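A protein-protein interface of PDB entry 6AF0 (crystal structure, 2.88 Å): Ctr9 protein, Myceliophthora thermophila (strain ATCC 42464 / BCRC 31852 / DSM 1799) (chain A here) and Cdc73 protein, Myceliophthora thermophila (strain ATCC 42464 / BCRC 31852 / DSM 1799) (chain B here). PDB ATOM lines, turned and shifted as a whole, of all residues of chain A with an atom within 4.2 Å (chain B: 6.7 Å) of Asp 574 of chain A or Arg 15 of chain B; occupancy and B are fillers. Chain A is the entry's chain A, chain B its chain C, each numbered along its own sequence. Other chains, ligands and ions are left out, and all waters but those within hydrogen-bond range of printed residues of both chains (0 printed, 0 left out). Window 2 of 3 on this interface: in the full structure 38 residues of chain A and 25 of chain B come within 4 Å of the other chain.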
ATOM      1  N   ASP A 572     -32.729  22.329   1.643  1.00  0.00           N
ATOM      2  CA  ASP A 572     -31.379  22.328   2.191  1.00  0.00           C
ATOM      3  C   ASP A 572     -30.497  23.191   1.296  1.00  0.00           C
ATOM      4  O   ASP A 572     -29.698  22.687   0.508  1.00  0.00           O
ATOM      5  CB  ASP A 572     -30.818  20.910   2.334  1.00  0.00           C
ATOM      6  CG  ASP A 572     -29.554  20.873   3.188  1.00  0.00           C
ATOM      7  OD1 ASP A 572     -28.955  21.955   3.442  1.00  0.00           O
ATOM      8  OD2 ASP A 572     -29.167  19.756   3.601  1.00  0.00           O
ATOM      9  N   ILE A 573     -30.654  24.502   1.440  1.00  0.00           N
ATOM     10  CA  ILE A 573     -29.983  25.474   0.564  1.00  0.00           C
ATOM     11  C   ILE A 573     -28.455  25.440   0.746  1.00  0.00           C
ATOM     12  O   ILE A 573     -27.703  25.622  -0.224  1.00  0.00           O
ATOM     13  CB  ILE A 573     -30.510  26.918   0.775  1.00  0.00           C
ATOM     14  CG1 ILE A 573     -32.049  26.972   0.766  1.00  0.00           C
ATOM     15  CG2 ILE A 573     -29.966  27.861  -0.289  1.00  0.00           C
ATOM     16  CD1 ILE A 573     -32.718  26.304  -0.417  1.00  0.00           C
ATOM     17  N   ASP A 574     -28.002  25.187   1.976  1.00  0.00           N
ATOM     18  CA  ASP A 574     -26.575  25.072   2.243  1.00  0.00           C
ATOM     19  C   ASP A 574     -25.983  23.863   1.518  1.00  0.00           C
ATOM     20  O   ASP A 574     -24.915  23.975   0.923  1.00  0.00           O
ATOM     21  CB  ASP A 574     -26.271  25.037   3.746  1.00  0.00           C
ATOM     22  CG  ASP A 574     -24.767  24.786   4.060  1.00  0.00           C
ATOM     23  OD1 ASP A 574     -23.928  24.918   3.143  1.00  0.00           O
ATOM     24  OD2 ASP A 574     -24.403  24.466   5.222  1.00  0.00           O
ATOM     25  N   ALA A 575     -26.673  22.724   1.540  1.00  0.00           N
ATOM     26  CA  ALA A 575     -26.245  21.558   0.734  1.00  0.00           C
ATOM     27  C   ALA A 575     -26.156  21.858  -0.777  1.00  0.00           C
ATOM     28  O   ALA A 575     -25.157  21.555  -1.433  1.00  0.00           O
ATOM     29  CB  ALA A 575     -27.163  20.377   0.960  1.00  0.00           C
ATOM     30  N   LEU A 576     -27.205  22.453  -1.324  1.00  0.00           N
ATOM     31  CA  LEU A 576     -27.212  22.848  -2.729  1.00  0.00           C
ATOM     32  C   LEU A 576     -26.164  23.926  -3.030  1.00  0.00           C
ATOM     33  O   LEU A 576     -25.646  24.021  -4.152  1.00  0.00           O
ATOM     34  CB  LEU A 576     -28.599  23.355  -3.123  1.00  0.00           C
ATOM     35  CG  LEU A 576     -29.621  22.295  -3.538  1.00  0.00           C
ATOM     36  CD1 LEU A 576     -29.843  21.207  -2.488  1.00  0.00           C
ATOM     37  CD2 LEU A 576     -30.927  22.995  -3.868  1.00  0.00           C
ATOM     38  N   LEU A 577     -25.866  24.751  -2.030  1.00  0.00           N
ATOM     39  CA  LEU A 577     -24.835  25.786  -2.169  1.00  0.00           C
ATOM     40  C   LEU A 577     -23.419  25.248  -1.931  1.00  0.00           C
ATOM     41  O   LEU A 577     -22.459  26.016  -1.990  1.00  0.00           O
ATOM     42  CB  LEU A 577     -25.111  26.952  -1.215  1.00  0.00           C
ATOM     43  CG  LEU A 577     -25.834  28.214  -1.708  1.00  0.00           C
ATOM     44  CD1 LEU A 577     -24.881  29.086  -2.518  1.00  0.00           C
ATOM     45  CD2 LEU A 577     -27.084  27.901  -2.512  1.00  0.00           C
ATOM     46  N   THR A 578     -23.306  23.956  -1.611  1.00  0.00           N
ATOM     47  CA  THR A 578     -22.015  23.255  -1.601  1.00  0.00           C
ATOM     48  C   THR A 578     -21.868  22.429  -2.880  1.00  0.00           C
ATOM     49  O   THR A 578     -20.851  22.512  -3.562  1.00  0.00           O
ATOM     50  CB  THR A 578     -21.798  22.362  -0.346  1.00  0.00           C
ATOM     51  OG1 THR A 578     -22.733  21.276  -0.330  1.00  0.00           O
ATOM     52  CG2 THR A 578     -21.922  23.183   0.943  1.00  0.00           C
ATOM     53  N   ARG A 607     -15.930  28.861   2.695  1.00  0.00           N
ATOM     54  CA  ARG A 607     -17.153  28.639   3.437  1.00  0.00           C
ATOM     55  C   ARG A 607     -17.266  27.170   3.893  1.00  0.00           C
ATOM     56  O   ARG A 607     -18.025  26.835   4.813  1.00  0.00           O
ATOM     57  CB  ARG A 607     -18.354  29.049   2.576  1.00  0.00           C
ATOM     58  CG  ARG A 607     -19.507  28.065   2.624  1.00  0.00           C
ATOM     59  CD  ARG A 607     -20.621  28.456   1.692  1.00  0.00           C
ATOM     60  NE  ARG A 607     -21.772  27.599   1.935  1.00  0.00           N
ATOM     61  CZ  ARG A 607     -23.008  27.876   1.544  1.00  0.00           C
ATOM     62  NH1 ARG A 607     -23.278  28.994   0.873  1.00  0.00           N
ATOM     63  NH2 ARG A 607     -23.983  27.032   1.828  1.00  0.00           N
ATOM     64  N   LEU B  12     -16.822  10.458   7.639  1.00  0.00           N
ATOM     65  CA  LEU B  12     -17.699  11.551   7.253  1.00  0.00           C
ATOM     66  C   LEU B  12     -18.225  12.274   8.490  1.00  0.00           C
ATOM     67  O   LEU B  12     -18.769  11.657   9.401  1.00  0.00           O
ATOM     68  CB  LEU B  12     -18.894  11.055   6.415  1.00  0.00           C
ATOM     69  CG  LEU B  12     -18.800  10.068   5.234  1.00  0.00           C
ATOM     70  CD1 LEU B  12     -18.299   8.679   5.613  1.00  0.00           C
ATOM     71  CD2 LEU B  12     -20.184   9.942   4.598  1.00  0.00           C
ATOM     72  N   ASP B  13     -18.045  13.587   8.509  1.00  0.00           N
ATOM     73  CA  ASP B  13     -18.839  14.498   9.344  1.00  0.00           C
ATOM     74  C   ASP B  13     -20.336  14.240   9.038  1.00  0.00           C
ATOM     75  O   ASP B  13     -20.687  13.957   7.894  1.00  0.00           O
ATOM     76  CB  ASP B  13     -18.431  15.939   8.971  1.00  0.00           C
ATOM     77  CG  ASP B  13     -19.077  17.015   9.834  1.00  0.00           C
ATOM     78  OD1 ASP B  13     -18.752  17.094  11.032  1.00  0.00           O
ATOM     79  OD2 ASP B  13     -19.864  17.826   9.303  1.00  0.00           O
ATOM     80  N   PRO B  14     -21.221  14.301  10.050  1.00  0.00           N
ATOM     81  CA  PRO B  14     -22.669  14.095   9.811  1.00  0.00           C
ATOM     82  C   PRO B  14     -23.300  15.025   8.775  1.00  0.00           C
ATOM     83  O   PRO B  14     -24.149  14.600   7.977  1.00  0.00           O
ATOM     84  CB  PRO B  14     -23.291  14.407  11.173  1.00  0.00           C
ATOM     85  CG  PRO B  14     -22.213  14.125  12.156  1.00  0.00           C
ATOM     86  CD  PRO B  14     -20.922  14.478  11.483  1.00  0.00           C
ATOM     87  N   ARG B  15     -22.908  16.295   8.839  1.00  0.00           N
ATOM     88  CA  ARG B  15     -23.377  17.311   7.904  1.00  0.00           C
ATOM     89  C   ARG B  15     -22.950  16.993   6.461  1.00  0.00           C
ATOM     90  O   ARG B  15     -23.764  17.069   5.538  1.00  0.00           O
ATOM     91  CB  ARG B  15     -22.861  18.687   8.337  1.00  0.00           C
ATOM     92  CG  ARG B  15     -23.274  19.836   7.439  1.00  0.00           C
ATOM     93  CD  ARG B  15     -24.785  19.928   7.305  1.00  0.00           C
ATOM     94  NE  ARG B  15     -25.187  20.950   6.342  1.00  0.00           N
ATOM     95  CZ  ARG B  15     -26.398  21.038   5.803  1.00  0.00           C
ATOM     96  NH1 ARG B  15     -27.347  20.172   6.133  1.00  0.00           N
ATOM     97  NH2 ARG B  15     -26.658  21.989   4.924  1.00  0.00           N
ATOM     98  N   LEU B  16     -21.679  16.635   6.282  1.00  0.00           N
ATOM     99  CA  LEU B  16     -21.155  16.200   4.973  1.00  0.00           C
ATOM    100  C   LEU B  16     -21.912  14.992   4.448  1.00  0.00           C
ATOM    101  O   LEU B  16     -22.253  14.945   3.270  1.00  0.00           O
ATOM    102  CB  LEU B  16     -19.661  15.853   5.047  1.00  0.00           C
ATOM    103  CG  LEU B  16     -18.675  17.011   4.868  1.00  0.00           C
ATOM    104  CD1 LEU B  16     -18.833  17.992   6.015  1.00  0.00           C
ATOM    105  CD2 LEU B  16     -17.229  16.530   4.769  1.00  0.00           C
ATOM    106  N   ALA B  17     -22.159  14.022   5.330  1.00  0.00           N
ATOM    107  CA  ALA B  17     -22.793  12.757   4.959  1.00  0.00           C
ATOM    108  C   ALA B  17     -24.175  12.978   4.381  1.00  0.00           C
ATOM    109  O   ALA B  17     -24.588  12.258   3.460  1.00  0.00           O
ATOM    110  CB  ALA B  17     -22.881  11.829   6.165  1.00  0.00           C
ATOM    111  N   GLN B  18     -24.888  13.962   4.932  1.00  0.00           N
ATOM    112  CA  GLN B  18     -26.239  14.271   4.458  1.00  0.00           C
ATOM    113  C   GLN B  18     -26.167  15.160   3.207  1.00  0.00           C
ATOM    114  O   GLN B  18     -26.979  15.025   2.293  1.00  0.00           O
ATOM    115  CB  GLN B  18     -27.135  14.848   5.581  1.00  0.00           C
ATOM    116  CG  GLN B  18     -28.420  14.036   5.795  1.00  0.00           C
ATOM    117  CD  GLN B  18     -28.144  12.556   6.086  1.00  0.00           C
ATOM    118  OE1 GLN B  18     -27.098  12.200   6.651  1.00  0.00           O
ATOM    119  NE2 GLN B  18     -29.074  11.684   5.690  1.00  0.00           N
ATOM    120  N   ILE B  19     -25.156  16.019   3.131  1.00  0.00           N
ATOM    121  CA  ILE B  19     -24.909  16.793   1.906  1.00  0.00           C
ATOM    122  C   ILE B  19     -24.655  15.850   0.717  1.00  0.00           C
ATOM    123  O   ILE B  19     -25.203  16.033  -0.374  1.00  0.00           O
ATOM    124  CB  ILE B  19     -23.737  17.788   2.081  1.00  0.00           C
ATOM    125  CG1 ILE B  19     -24.173  18.976   2.939  1.00  0.00           C
ATOM    126  CG2 ILE B  19     -23.271  18.327   0.742  1.00  0.00           C
ATOM    127  CD1 ILE B  19     -23.119  20.051   3.136  1.00  0.00           C
ATOM    128  N   TYR B  20     -23.827  14.836   0.941  1.00  0.00           N
ATOM    129  CA  TYR B  20     -23.534  13.833  -0.074  1.00  0.00           C
ATOM    130  C   TYR B  20     -24.754  12.984  -0.396  1.00  0.00           C
ATOM    131  O   TYR B  20     -24.873  12.448  -1.498  1.00  0.00           O
ATOM    132  CB  TYR B  20     -22.405  12.912   0.394  1.00  0.00           C
ATOM    133  CG  TYR B  20     -21.035  13.555   0.570  1.00  0.00           C
ATOM    134  CD1 TYR B  20     -19.971  12.824   1.093  1.00  0.00           C
ATOM    135  CD2 TYR B  20     -20.800  14.885   0.227  1.00  0.00           C
ATOM    136  CE1 TYR B  20     -18.719  13.389   1.248  1.00  0.00           C
ATOM    137  CE2 TYR B  20     -19.551  15.455   0.389  1.00  0.00           C
ATOM    138  CZ  TYR B  20     -18.509  14.709   0.900  1.00  0.00           C
ATOM    139  OH  TYR B  20     -17.259  15.301   1.064  1.00  0.00           O
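Among the printed residues, 5 pairs touch across the chains.
Among the printed residues, Asp or Glu carboxylates within 4 Å of a Lys or Arg side-chain nitrogen of the other chain: Asp 572 of chain A with Arg 15 of chain B and Asp 574 of chain A with Arg 15 of chain B.
Ile 573 of chain A touches none of the printed residues of chain B.
Of chain B, only Arg 15 comes within 4 Å of Asp 574 of chain A.
Printed residues of chain B within 4 Å of Thr 578 of chain A: Ile 19.
Of chain A, only Asp 572 (2.7 Å), Asp 574 (3.3 Å) and Ala 575 (3.5 Å) come within 4 Å of Arg 15 of chain B.
Printed residues of chain A within 4 Å of Ile 19 of chain B: Ala 575 and Thr 578.
The nearest residue of chain B that does not touch Asp 574 of chain A is Ile 19 of chain B (4.8 Å).
The nearest printed residue of chain A that does not touch Arg 15 of chain B is Ile 573 of chain A (5.7 Å).
Ala 575 of chain A touches Ile 19 of chain B.
Thr 578 of chain A touches Ile 19 of chain B.
The backbone carbonyl oxygen (O) of Ala 575 of chain A sits at hydrogen-bond distance from the side-chain hydroxyl (OG1) of Thr 578 of chain A (2.7 Å).
OD1 of Asp 572 of chain A lies within hydrogen-bond range of N of Ala 575 of chain A (3.1 Å).
The guanidinium group of Arg 607 of chain A is in salt-bridge range of the side-chain carboxylate of Asp 574 of chain A (2.5 Å).
OD2 of Asp 13 of chain B sits close to N of Arg 15 of chain B.
OD1 of Asp 572 of chain A is in salt-bridge range of NH2 of Arg 15 of chain B (2.7 Å).
OD2 of Asp 574 of chain A lies within salt-bridge range of NH2 of Arg 15 of chain B (3.4 Å).
The backbone NH (N) of Ala 575 of chain A lies close to the guanidinium group (NH2) of Arg 15 of chain B (3.5 Å).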
